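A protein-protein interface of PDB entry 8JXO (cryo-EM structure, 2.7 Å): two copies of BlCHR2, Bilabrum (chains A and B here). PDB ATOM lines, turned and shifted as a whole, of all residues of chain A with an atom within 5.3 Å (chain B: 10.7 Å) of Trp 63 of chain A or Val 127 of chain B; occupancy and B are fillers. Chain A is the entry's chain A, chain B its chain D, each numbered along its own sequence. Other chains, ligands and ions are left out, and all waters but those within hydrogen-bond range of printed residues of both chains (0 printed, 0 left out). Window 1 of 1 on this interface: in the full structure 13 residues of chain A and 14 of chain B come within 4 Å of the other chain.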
ATOM      1  N   ALA A  39      12.311  36.671  -2.600  1.00  0.00           N
ATOM      2  CA  ALA A  39      11.610  35.612  -1.882  1.00  0.00           C
ATOM      3  C   ALA A  39      10.717  36.187  -0.815  1.00  0.00           C
ATOM      4  O   ALA A  39       9.573  35.780  -0.686  1.00  0.00           O
ATOM      5  CB  ALA A  39      12.587  34.628  -1.273  1.00  0.00           C
ATOM      6  N   THR A  42       7.673  37.839  -2.507  1.00  0.00           N
ATOM      7  CA  THR A  42       6.705  36.883  -3.020  1.00  0.00           C
ATOM      8  C   THR A  42       5.936  36.230  -1.890  1.00  0.00           C
ATOM      9  O   THR A  42       4.735  36.042  -1.995  1.00  0.00           O
ATOM     10  CB  THR A  42       7.333  35.801  -3.916  1.00  0.00           C
ATOM     11  OG1 THR A  42       8.538  35.316  -3.326  1.00  0.00           O
ATOM     12  CG2 THR A  42       7.638  36.367  -5.286  1.00  0.00           C
ATOM     13  N   ALA A  43       6.618  35.890  -0.805  1.00  0.00           N
ATOM     14  CA  ALA A  43       5.953  35.269   0.331  1.00  0.00           C
ATOM     15  C   ALA A  43       5.054  36.243   1.059  1.00  0.00           C
ATOM     16  O   ALA A  43       3.892  35.935   1.315  1.00  0.00           O
ATOM     17  CB  ALA A  43       6.975  34.694   1.290  1.00  0.00           C
ATOM     18  N   PRO A  58       1.846  31.526  -2.162  1.00  0.00           N
ATOM     19  CA  PRO A  58       2.467  31.962  -3.414  1.00  0.00           C
ATOM     20  C   PRO A  58       2.586  30.814  -4.394  1.00  0.00           C
ATOM     21  O   PRO A  58       2.939  29.710  -3.988  1.00  0.00           O
ATOM     22  CB  PRO A  58       3.858  32.424  -2.975  1.00  0.00           C
ATOM     23  CG  PRO A  58       3.737  32.699  -1.516  1.00  0.00           C
ATOM     24  CD  PRO A  58       2.733  31.713  -1.005  1.00  0.00           C
ATOM     25  N   PRO A  59       2.286  31.062  -5.674  1.00  0.00           N
ATOM     26  CA  PRO A  59       2.434  30.021  -6.692  1.00  0.00           C
ATOM     27  C   PRO A  59       3.854  29.470  -6.733  1.00  0.00           C
ATOM     28  O   PRO A  59       4.794  30.172  -6.374  1.00  0.00           O
ATOM     29  CB  PRO A  59       2.099  30.755  -7.990  1.00  0.00           C
ATOM     30  CG  PRO A  59       1.192  31.858  -7.571  1.00  0.00           C
ATOM     31  CD  PRO A  59       1.655  32.282  -6.208  1.00  0.00           C
ATOM     32  N   GLU A  60       4.019  28.232  -7.175  1.00  0.00           N
ATOM     33  CA  GLU A  60       5.341  27.616  -7.190  1.00  0.00           C
ATOM     34  C   GLU A  60       6.278  28.288  -8.174  1.00  0.00           C
ATOM     35  O   GLU A  60       7.494  28.181  -8.047  1.00  0.00           O
ATOM     36  CB  GLU A  60       5.235  26.130  -7.511  1.00  0.00           C
ATOM     37  CG  GLU A  60       5.342  25.227  -6.296  1.00  0.00           C
ATOM     38  CD  GLU A  60       4.511  23.969  -6.436  1.00  0.00           C
ATOM     39  OE1 GLU A  60       4.689  23.251  -7.442  1.00  0.00           O
ATOM     40  OE2 GLU A  60       3.678  23.703  -5.546  1.00  0.00           O
ATOM     41  N   GLU A  61       5.722  28.977  -9.160  1.00  0.00           N
ATOM     42  CA  GLU A  61       6.538  29.672 -10.141  1.00  0.00           C
ATOM     43  C   GLU A  61       7.008  31.009  -9.600  1.00  0.00           C
ATOM     44  O   GLU A  61       7.943  31.599 -10.135  1.00  0.00           O
ATOM     45  CB  GLU A  61       5.754  29.869 -11.433  1.00  0.00           C
ATOM     46  CG  GLU A  61       4.686  28.818 -11.673  1.00  0.00           C
ATOM     47  CD  GLU A  61       3.288  29.348 -11.429  1.00  0.00           C
ATOM     48  OE1 GLU A  61       2.461  28.605 -10.860  1.00  0.00           O
ATOM     49  OE2 GLU A  61       3.018  30.506 -11.804  1.00  0.00           O
ATOM     50  N   ASN A  62       6.364  31.499  -8.549  1.00  0.00           N
ATOM     51  CA  ASN A  62       6.807  32.739  -7.933  1.00  0.00           C
ATOM     52  C   ASN A  62       8.143  32.506  -7.259  1.00  0.00           C
ATOM     53  O   ASN A  62       8.804  33.458  -6.870  1.00  0.00           O
ATOM     54  CB  ASN A  62       5.773  33.245  -6.932  1.00  0.00           C
ATOM     55  CG  ASN A  62       4.658  34.023  -7.595  1.00  0.00           C
ATOM     56  OD1 ASN A  62       4.374  33.837  -8.776  1.00  0.00           O
ATOM     57  ND2 ASN A  62       4.015  34.901  -6.834  1.00  0.00           N
ATOM     58  N   TRP A  63       8.537  31.246  -7.100  1.00  0.00           N
ATOM     59  CA  TRP A  63       9.832  30.902  -6.524  1.00  0.00           C
ATOM     60  C   TRP A  63      10.921  30.624  -7.540  1.00  0.00           C
ATOM     61  O   TRP A  63      12.084  30.549  -7.178  1.00  0.00           O
ATOM     62  CB  TRP A  63       9.680  29.695  -5.606  1.00  0.00           C
ATOM     63  CG  TRP A  63       8.640  29.870  -4.556  1.00  0.00           C
ATOM     64  CD1 TRP A  63       7.456  29.206  -4.460  1.00  0.00           C
ATOM     65  CD2 TRP A  63       8.690  30.768  -3.443  1.00  0.00           C
ATOM     66  NE1 TRP A  63       6.762  29.636  -3.356  1.00  0.00           N
ATOM     67  CE2 TRP A  63       7.499  30.595  -2.716  1.00  0.00           C
ATOM     68  CE3 TRP A  63       9.626  31.702  -2.991  1.00  0.00           C
ATOM     69  CZ2 TRP A  63       7.221  31.318  -1.563  1.00  0.00           C
ATOM     70  CZ3 TRP A  63       9.348  32.417  -1.849  1.00  0.00           C
ATOM     71  CH2 TRP A  63       8.155  32.225  -1.149  1.00  0.00           C
ATOM     72  N   LEU A  64      10.560  30.455  -8.806  1.00  0.00           N
ATOM     73  CA  LEU A  64      11.563  30.261  -9.839  1.00  0.00           C
ATOM     74  C   LEU A  64      12.485  31.463  -9.862  1.00  0.00           C
ATOM     75  O   LEU A  64      13.692  31.301  -9.796  1.00  0.00           O
ATOM     76  CB  LEU A  64      10.907  30.067 -11.203  1.00  0.00           C
ATOM     77  CG  LEU A  64      11.174  28.756 -11.937  1.00  0.00           C
ATOM     78  CD1 LEU A  64      10.776  28.885 -13.397  1.00  0.00           C
ATOM     79  CD2 LEU A  64      12.634  28.353 -11.812  1.00  0.00           C
ATOM     80  N   SER A  65      11.958  32.685  -9.888  1.00  0.00           N
ATOM     81  CA  SER A  65      12.804  33.900  -9.945  1.00  0.00           C
ATOM     82  C   SER A  65      13.745  34.084  -8.719  1.00  0.00           C
ATOM     83  O   SER A  65      14.955  34.162  -8.928  1.00  0.00           O
ATOM     84  CB  SER A  65      11.986  35.162 -10.257  1.00  0.00           C
ATOM     85  OG  SER A  65      12.559  35.887 -11.329  1.00  0.00           O
ATOM     86  N   PRO A  66      13.218  34.191  -7.446  1.00  0.00           N
ATOM     87  CA  PRO A  66      14.177  34.245  -6.332  1.00  0.00           C
ATOM     88  C   PRO A  66      15.105  33.061  -6.403  1.00  0.00           C
ATOM     89  O   PRO A  66      16.306  33.211  -6.182  1.00  0.00           O
ATOM     90  CB  PRO A  66      13.289  34.079  -5.106  1.00  0.00           C
ATOM     91  CG  PRO A  66      11.974  34.616  -5.511  1.00  0.00           C
ATOM     92  CD  PRO A  66      11.823  34.230  -6.939  1.00  0.00           C
ATOM     93  N   GLY A  67      14.555  31.895  -6.711  1.00  0.00           N
ATOM     94  CA  GLY A  67      15.345  30.684  -6.793  1.00  0.00           C
ATOM     95  C   GLY A  67      16.620  30.842  -7.567  1.00  0.00           C
ATOM     96  O   GLY A  67      17.668  30.607  -7.015  1.00  0.00           O
ATOM     97  N   ILE A  68      16.538  31.240  -8.829  1.00  0.00           N
ATOM     98  CA  ILE A  68      17.726  31.378  -9.665  1.00  0.00           C
ATOM     99  C   ILE A  68      18.748  32.307  -9.038  1.00  0.00           C
ATOM    100  O   ILE A  68      19.908  31.953  -8.919  1.00  0.00           O
ATOM    101  CB  ILE A  68      17.383  31.900 -11.068  1.00  0.00           C
ATOM    102  CG1 ILE A  68      16.293  31.047 -11.696  1.00  0.00           C
ATOM    103  CG2 ILE A  68      18.614  31.896 -11.961  1.00  0.00           C
ATOM    104  CD1 ILE A  68      15.369  31.830 -12.597  1.00  0.00           C
ATOM    105  N   CYS B 109      17.093  11.635  -3.592  1.00  0.00           N
ATOM    106  CA  CYS B 109      16.528  12.723  -2.799  1.00  0.00           C
ATOM    107  C   CYS B 109      15.570  13.642  -3.534  1.00  0.00           C
ATOM    108  O   CYS B 109      14.466  13.913  -3.050  1.00  0.00           O
ATOM    109  CB  CYS B 109      17.644  13.473  -2.106  1.00  0.00           C
ATOM    110  SG  CYS B 109      18.143  12.678  -0.600  1.00  0.00           S
ATOM    111  N   PRO B 110      16.030  14.250  -4.652  1.00  0.00           N
ATOM    112  CA  PRO B 110      14.944  14.957  -5.324  1.00  0.00           C
ATOM    113  C   PRO B 110      13.708  14.123  -5.606  1.00  0.00           C
ATOM    114  O   PRO B 110      12.632  14.704  -5.654  1.00  0.00           O
ATOM    115  CB  PRO B 110      15.607  15.419  -6.602  1.00  0.00           C
ATOM    116  CG  PRO B 110      16.984  15.730  -6.135  1.00  0.00           C
ATOM    117  CD  PRO B 110      17.124  15.225  -4.713  1.00  0.00           C
ATOM    118  N   VAL B 113      11.742  13.708  -1.656  1.00  0.00           N
ATOM    119  CA  VAL B 113      11.104  14.924  -1.179  1.00  0.00           C
ATOM    120  C   VAL B 113       9.903  15.222  -2.050  1.00  0.00           C
ATOM    121  O   VAL B 113       8.857  15.598  -1.543  1.00  0.00           O
ATOM    122  CB  VAL B 113      12.074  16.113  -1.155  1.00  0.00           C
ATOM    123  CG1 VAL B 113      11.457  17.288  -0.417  1.00  0.00           C
ATOM    124  CG2 VAL B 113      13.354  15.712  -0.457  1.00  0.00           C
ATOM    125  N   LEU B 114      10.023  15.027  -3.356  1.00  0.00           N
ATOM    126  CA  LEU B 114       8.876  15.217  -4.232  1.00  0.00           C
ATOM    127  C   LEU B 114       7.753  14.292  -3.811  1.00  0.00           C
ATOM    128  O   LEU B 114       6.632  14.735  -3.663  1.00  0.00           O
ATOM    129  CB  LEU B 114       9.248  14.951  -5.683  1.00  0.00           C
ATOM    130  CG  LEU B 114       9.108  16.118  -6.658  1.00  0.00           C
ATOM    131  CD1 LEU B 114       8.639  15.612  -8.010  1.00  0.00           C
ATOM    132  CD2 LEU B 114       8.163  17.179  -6.119  1.00  0.00           C
ATOM    133  N   CYS B 117       6.108  15.522  -0.640  1.00  0.00           N
ATOM    134  CA  CYS B 117       5.325  16.708  -0.938  1.00  0.00           C
ATOM    135  C   CYS B 117       4.083  16.480  -1.785  1.00  0.00           C
ATOM    136  O   CYS B 117       3.137  17.234  -1.687  1.00  0.00           O
ATOM    137  CB  CYS B 117       6.216  17.758  -1.584  1.00  0.00           C
ATOM    138  SG  CYS B 117       7.442  18.477  -0.473  1.00  0.00           S
ATOM    139  N   ILE B 118       4.076  15.458  -2.625  1.00  0.00           N
ATOM    140  CA  ILE B 118       2.896  15.158  -3.420  1.00  0.00           C
ATOM    141  C   ILE B 118       1.870  14.415  -2.578  1.00  0.00           C
ATOM    142  O   ILE B 118       0.706  14.810  -2.527  1.00  0.00           O
ATOM    143  CB  ILE B 118       3.253  14.346  -4.682  1.00  0.00           C
ATOM    144  CG1 ILE B 118       4.034  15.209  -5.669  1.00  0.00           C
ATOM    145  CG2 ILE B 118       2.007  13.820  -5.371  1.00  0.00           C
ATOM    146  CD1 ILE B 118       4.790  14.405  -6.702  1.00  0.00           C
ATOM    147  N   LEU B 122       2.071  18.778   0.445  1.00  0.00           N
ATOM    148  CA  LEU B 122       2.816  19.853   1.065  1.00  0.00           C
ATOM    149  C   LEU B 122       3.042  20.872  -0.023  1.00  0.00           C
ATOM    150  O   LEU B 122       3.234  20.514  -1.179  1.00  0.00           O
ATOM    151  CB  LEU B 122       4.159  19.345   1.578  1.00  0.00           C
ATOM    152  CG  LEU B 122       4.301  18.888   3.026  1.00  0.00           C
ATOM    153  CD1 LEU B 122       2.954  18.830   3.722  1.00  0.00           C
ATOM    154  CD2 LEU B 122       5.000  17.542   3.075  1.00  0.00           C
ATOM    155  N   ARG B 123       3.024  22.146   0.335  1.00  0.00           N
ATOM    156  CA  ARG B 123       3.210  23.193  -0.652  1.00  0.00           C
ATOM    157  C   ARG B 123       4.660  23.299  -1.081  1.00  0.00           C
ATOM    158  O   ARG B 123       5.521  22.627  -0.518  1.00  0.00           O
ATOM    159  CB  ARG B 123       2.724  24.532  -0.105  1.00  0.00           C
ATOM    160  CG  ARG B 123       1.247  24.557   0.244  1.00  0.00           C
ATOM    161  CD  ARG B 123       1.028  25.147   1.623  1.00  0.00           C
ATOM    162  NE  ARG B 123       1.297  26.581   1.648  1.00  0.00           N
ATOM    163  CZ  ARG B 123       1.366  27.306   2.756  1.00  0.00           C
ATOM    164  NH1 ARG B 123       1.188  26.730   3.937  1.00  0.00           N
ATOM    165  NH2 ARG B 123       1.614  28.607   2.688  1.00  0.00           N
ATOM    166  N   TYR B 124       4.934  24.139  -2.075  1.00  0.00           N
ATOM    167  CA  TYR B 124       6.299  24.332  -2.560  1.00  0.00           C
ATOM    168  C   TYR B 124       6.985  23.013  -2.868  1.00  0.00           C
ATOM    169  O   TYR B 124       8.155  22.837  -2.548  1.00  0.00           O
ATOM    170  CB  TYR B 124       7.135  25.139  -1.558  1.00  0.00           C
ATOM    171  CG  TYR B 124       6.364  26.180  -0.782  1.00  0.00           C
ATOM    172  CD1 TYR B 124       5.680  27.199  -1.432  1.00  0.00           C
ATOM    173  CD2 TYR B 124       6.327  26.147   0.606  1.00  0.00           C
ATOM    174  CE1 TYR B 124       4.973  28.150  -0.720  1.00  0.00           C
ATOM    175  CE2 TYR B 124       5.626  27.095   1.321  1.00  0.00           C
ATOM    176  CZ  TYR B 124       4.951  28.092   0.655  1.00  0.00           C
ATOM    177  OH  TYR B 124       4.255  29.038   1.369  1.00  0.00           O
ATOM    178  N   LYS B 125       6.266  22.088  -3.493  1.00  0.00           N
ATOM    179  CA  LYS B 125       6.830  20.779  -3.791  1.00  0.00           C
ATOM    180  C   LYS B 125       8.125  20.870  -4.556  1.00  0.00           C
ATOM    181  O   LYS B 125       9.131  20.284  -4.163  1.00  0.00           O
ATOM    182  CB  LYS B 125       5.831  19.956  -4.600  1.00  0.00           C
ATOM    183  CG  LYS B 125       4.383  20.363  -4.399  1.00  0.00           C
ATOM    184  CD  LYS B 125       3.450  19.190  -4.637  1.00  0.00           C
ATOM    185  CE  LYS B 125       2.027  19.525  -4.219  1.00  0.00           C
ATOM    186  NZ  LYS B 125       1.215  18.300  -3.980  1.00  0.00           N
ATOM    187  N   LEU B 126       8.089  21.589  -5.672  1.00  0.00           N
ATOM    188  CA  LEU B 126       9.267  21.700  -6.515  1.00  0.00           C
ATOM    189  C   LEU B 126      10.355  22.472  -5.814  1.00  0.00           C
ATOM    190  O   LEU B 126      11.498  22.073  -5.870  1.00  0.00           O
ATOM    191  CB  LEU B 126       8.924  22.345  -7.853  1.00  0.00           C
ATOM    192  CG  LEU B 126       8.748  21.366  -9.017  1.00  0.00           C
ATOM    193  CD1 LEU B 126       9.674  20.170  -8.859  1.00  0.00           C
ATOM    194  CD2 LEU B 126       7.302  20.914  -9.125  1.00  0.00           C
ATOM    195  N   VAL B 127      10.004  23.556  -5.136  1.00  0.00           N
ATOM    196  CA  VAL B 127      10.995  24.307  -4.377  1.00  0.00           C
ATOM    197  C   VAL B 127      11.774  23.378  -3.464  1.00  0.00           C
ATOM    198  O   VAL B 127      12.985  23.285  -3.581  1.00  0.00           O
ATOM    199  CB  VAL B 127      10.349  25.421  -3.538  1.00  0.00           C
ATOM    200  CG1 VAL B 127      11.407  26.210  -2.782  1.00  0.00           C
ATOM    201  CG2 VAL B 127       9.525  26.338  -4.426  1.00  0.00           C
ATOM    202  N   PHE B 128      11.083  22.675  -2.574  1.00  0.00           N
ATOM    203  CA  PHE B 128      11.741  21.747  -1.656  1.00  0.00           C
ATOM    204  C   PHE B 128      12.614  20.740  -2.382  1.00  0.00           C
ATOM    205  O   PHE B 128      13.766  20.535  -2.009  1.00  0.00           O
ATOM    206  CB  PHE B 128      10.701  20.999  -0.828  1.00  0.00           C
ATOM    207  CG  PHE B 128      10.139  21.797   0.310  1.00  0.00           C
ATOM    208  CD1 PHE B 128      10.976  22.437   1.202  1.00  0.00           C
ATOM    209  CD2 PHE B 128       8.772  21.899   0.490  1.00  0.00           C
ATOM    210  CE1 PHE B 128      10.459  23.171   2.249  1.00  0.00           C
ATOM    211  CE2 PHE B 128       8.248  22.632   1.533  1.00  0.00           C
ATOM    212  CZ  PHE B 128       9.092  23.270   2.415  1.00  0.00           C
ATOM    213  N   SER B 129      12.079  20.116  -3.423  1.00  0.00           N
ATOM    214  CA  SER B 129      12.827  19.087  -4.133  1.00  0.00           C
ATOM    215  C   SER B 129      14.103  19.604  -4.774  1.00  0.00           C
ATOM    216  O   SER B 129      15.107  18.906  -4.795  1.00  0.00           O
ATOM    217  CB  SER B 129      11.943  18.425  -5.184  1.00  0.00           C
ATOM    218  OG  SER B 129      12.191  18.955  -6.472  1.00  0.00           O
ATOM    219  N   SER B 130      14.071  20.826  -5.292  1.00  0.00           N
ATOM    220  CA  SER B 130      15.242  21.397  -5.944  1.00  0.00           C
ATOM    221  C   SER B 130      16.237  21.861  -4.901  1.00  0.00           C
ATOM    222  O   SER B 130      17.451  21.804  -5.112  1.00  0.00           O
ATOM    223  CB  SER B 130      14.836  22.556  -6.845  1.00  0.00           C
ATOM    224  OG  SER B 130      14.316  23.633  -6.090  1.00  0.00           O
ATOM    225  N   SER B 131      15.731  22.319  -3.766  1.00  0.00           N
ATOM    226  CA  SER B 131      16.610  22.730  -2.698  1.00  0.00           C
ATOM    227  C   SER B 131      17.408  21.519  -2.263  1.00  0.00           C
ATOM    228  O   SER B 131      18.618  21.601  -2.096  1.00  0.00           O
ATOM    229  CB  SER B 131      15.808  23.283  -1.526  1.00  0.00           C
ATOM    230  OG  SER B 131      16.125  22.606  -0.324  1.00  0.00           O
ATOM    231  N   ILE B 132      16.738  20.382  -2.100  1.00  0.00           N
ATOM    232  CA  ILE B 132      17.437  19.195  -1.627  1.00  0.00           C
ATOM    233  C   ILE B 132      18.441  18.716  -2.665  1.00  0.00           C
ATOM    234  O   ILE B 132      19.545  18.323  -2.311  1.00  0.00           O
ATOM    235  CB  ILE B 132      16.454  18.105  -1.146  1.00  0.00           C
ATOM    236  CG1 ILE B 132      16.390  18.106   0.382  1.00  0.00           C
ATOM    237  CG2 ILE B 132      16.848  16.721  -1.620  1.00  0.00           C
ATOM    238  CD1 ILE B 132      15.356  19.046   0.961  1.00  0.00           C
ATOM    239  N   ALA B 133      18.106  18.815  -3.946  1.00  0.00           N
ATOM    240  CA  ALA B 133      19.060  18.451  -4.987  1.00  0.00           C
ATOM    241  C   ALA B 133      20.301  19.318  -4.899  1.00  0.00           C
ATOM    242  O   ALA B 133      21.413  18.826  -5.025  1.00  0.00           O
ATOM    243  CB  ALA B 133      18.429  18.584  -6.355  1.00  0.00           C
ATOM    244  N   CYS B 134      20.118  20.612  -4.669  1.00  0.00           N
ATOM    245  CA  CYS B 134      21.249  21.524  -4.555  1.00  0.00           C
ATOM    246  C   CYS B 134      22.074  21.293  -3.303  1.00  0.00           C
ATOM    247  O   CYS B 134      23.284  21.449  -3.329  1.00  0.00           O
ATOM    248  CB  CYS B 134      20.773  22.972  -4.596  1.00  0.00           C
ATOM    249  SG  CYS B 134      20.125  23.492  -6.200  1.00  0.00           S
ATOM    250  N   LEU B 135      21.432  20.912  -2.205  1.00  0.00           N
ATOM    251  CA  LEU B 135      22.147  20.657  -0.958  1.00  0.00           C
ATOM    252  C   LEU B 135      22.862  19.334  -1.010  1.00  0.00           C
ATOM    253  O   LEU B 135      23.808  19.108  -0.267  1.00  0.00           O
ATOM    254  CB  LEU B 135      21.193  20.662   0.226  1.00  0.00           C
ATOM    255  CG  LEU B 135      20.472  21.977   0.463  1.00  0.00           C
ATOM    256  CD1 LEU B 135      19.281  21.762   1.380  1.00  0.00           C
ATOM    257  CD2 LEU B 135      21.430  23.025   0.994  1.00  0.00           C
ATOM    258  N   GLY B 160      21.552  25.580   4.643  1.00  0.00           N
ATOM    259  CA  GLY B 160      20.402  25.301   3.806  1.00  0.00           C
ATOM    260  C   GLY B 160      19.613  24.082   4.236  1.00  0.00           C
ATOM    261  O   GLY B 160      18.407  24.070   4.097  1.00  0.00           O
ATOM    262  N   CYS B 163      17.557  25.193   7.131  1.00  0.00           N
ATOM    263  CA  CYS B 163      16.494  26.052   6.623  1.00  0.00           C
ATOM    264  C   CYS B 163      15.394  25.251   5.950  1.00  0.00           C
ATOM    265  O   CYS B 163      14.218  25.466   6.225  1.00  0.00           O
ATOM    266  CB  CYS B 163      17.056  27.067   5.632  1.00  0.00           C
ATOM    267  SG  CYS B 163      17.942  28.446   6.390  1.00  0.00           S
ATOM    268  N   ALA B 164      15.766  24.324   5.076  1.00  0.00           N
ATOM    269  CA  ALA B 164      14.781  23.513   4.370  1.00  0.00           C
ATOM    270  C   ALA B 164      14.085  22.575   5.325  1.00  0.00           C
ATOM    271  O   ALA B 164      12.915  22.278   5.151  1.00  0.00           O
ATOM    272  CB  ALA B 164      15.438  22.728   3.254  1.00  0.00           C
ATOM    273  N   GLY B 165      14.799  22.106   6.337  1.00  0.00           N
ATOM    274  CA  GLY B 165      14.202  21.232   7.318  1.00  0.00           C
ATOM    275  C   GLY B 165      13.165  21.971   8.115  1.00  0.00           C
ATOM    276  O   GLY B 165      12.088  21.453   8.353  1.00  0.00           O
ATOM    277  N   ALA B 167      11.495  24.676   7.190  1.00  0.00           N
ATOM    278  CA  ALA B 167      10.379  24.936   6.301  1.00  0.00           C
ATOM    279  C   ALA B 167       9.531  23.691   6.086  1.00  0.00           C
ATOM    280  O   ALA B 167       8.308  23.775   6.065  1.00  0.00           O
ATOM    281  CB  ALA B 167      10.877  25.483   4.980  1.00  0.00           C
ATOM    282  N   LEU B 168      10.170  22.538   5.934  1.00  0.00           N
ATOM    283  CA  LEU B 168       9.431  21.296   5.756  1.00  0.00           C
ATOM    284  C   LEU B 168       8.630  20.980   6.995  1.00  0.00           C
ATOM    285  O   LEU B 168       7.453  20.694   6.893  1.00  0.00           O
ATOM    286  CB  LEU B 168      10.358  20.132   5.425  1.00  0.00           C
ATOM    287  CG  LEU B 168       9.994  19.230   4.243  1.00  0.00           C
ATOM    288  CD1 LEU B 168      10.120  17.774   4.643  1.00  0.00           C
ATOM    289  CD2 LEU B 168       8.603  19.511   3.703  1.00  0.00           C
ATOM    290  N   GLU B 171       5.571  22.993   7.041  1.00  0.00           N
ATOM    291  CA  GLU B 171       4.594  22.512   6.069  1.00  0.00           C
ATOM    292  C   GLU B 171       3.815  21.287   6.536  1.00  0.00           C
ATOM    293  O   GLU B 171       2.598  21.254   6.419  1.00  0.00           O
ATOM    294  CB  GLU B 171       5.264  22.221   4.729  1.00  0.00           C
ATOM    295  CG  GLU B 171       4.750  23.078   3.590  1.00  0.00           C
ATOM    296  CD  GLU B 171       5.034  24.543   3.816  1.00  0.00           C
ATOM    297  OE1 GLU B 171       4.071  25.336   3.870  1.00  0.00           O
ATOM    298  OE2 GLU B 171       6.222  24.905   3.948  1.00  0.00           O
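The side-chain hydroxyl (OG) of Ser 130 of chain B lies within hydrogen-bond range of the backbone carbonyl oxygen (O) of Val 127 of chain B. The backbone carbonyl oxygen (O) of Leu 126 of chain B is in hydrogen-bond range of the side-chain hydroxyl (OG) of Ser 129 of chain B (3.3 Å). The backbone carbonyl oxygen (O) of Cys 117 of chain B lies within hydrogen-bond range of the side-chain amino group (NZ) of Lys 125 of chain B (3.2 Å). The side-chain hydroxyl of Ser 130 of chain B lies within hydrogen-bond range of the backbone carbonyl oxygen of Leu 126 of chain B, at 3.2 Å. OH of Tyr 124 of chain B sits at hydrogen-bond distance from NH2 of Arg 123 of chain B (3.0 Å).
Tyr 124 of chain B touches Pro 58 of chain A (OH to CD, 3.9 Å). Tyr 124 of chain B touches Glu 60 of chain A. Glu 60 of chain A touches Lys 125 of chain B. Glu 60 of chain A touches Leu 126 of chain B. NE1 of Trp 63 of chain A touches CD1 of Tyr 124 of chain B, 3.3 Å away. Trp 63 of chain A touches Val 127 of chain B (CD1 to CG2, 3.5 Å).
No residue of chain B comes within 4 Å of Thr 42 of chain A. Ala 43 of chain A touches none of the printed residues of chain B. Pro 58 of chain A touches one residue of chain B. Of chain B, only Tyr 124 (3.7 Å), Lys 125 (3.6 Å) and Leu 126 (3.9 Å) come within 4 Å of Glu 60 of chain A. No residue of chain B comes within 4 Å of Asn 62 of chain A. Trp 63 of chain A touches just these residues of chain B: Tyr 124 and Val 127. No residue of chain B comes within 4 Å of Leu 64 of chain A. Pro 110 of chain B touches none of the printed residues of chain A. Printed residues of chain A within 4 Å of Tyr 124 of chain B: Pro 58 (3.9 Å), Glu 60 (3.7 Å) and Trp 63 (3.3 Å). Printed residues of chain A within 4 Å of Lys 125 of chain B: Glu 60 (3.6 Å). Printed residues of chain A within 4 Å of Leu 126 of chain B: Glu 60. Val 127 of chain B touches one residue of chain A. The nearest residue of chain B that does not touch Trp 63 of chain A is Arg 123 of chain B (7.1 Å). The nearest printed residue of chain A that does not touch Tyr 124 of chain B is Pro 59 of chain A (5.8 Å).
No position is printed for both chains.
Of the 14 printed residues of chain A, 3 touch a printed residue of chain B. Hydrophobic or aromatic side chains of chain A that line the printed part of chain B: Pro 58 and Trp 63. Of the 27 printed residues of chain B, 4 touch a printed residue of chain A. Hydrophobic or aromatic side chains of chain B within 4 Å of the printed part of chain A: Tyr 124, Leu 126 and Val 127. Among the printed residues, no Asp or Glu carboxylate lies within 4 Å of a Lys or Arg side-chain nitrogen of the other chain.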
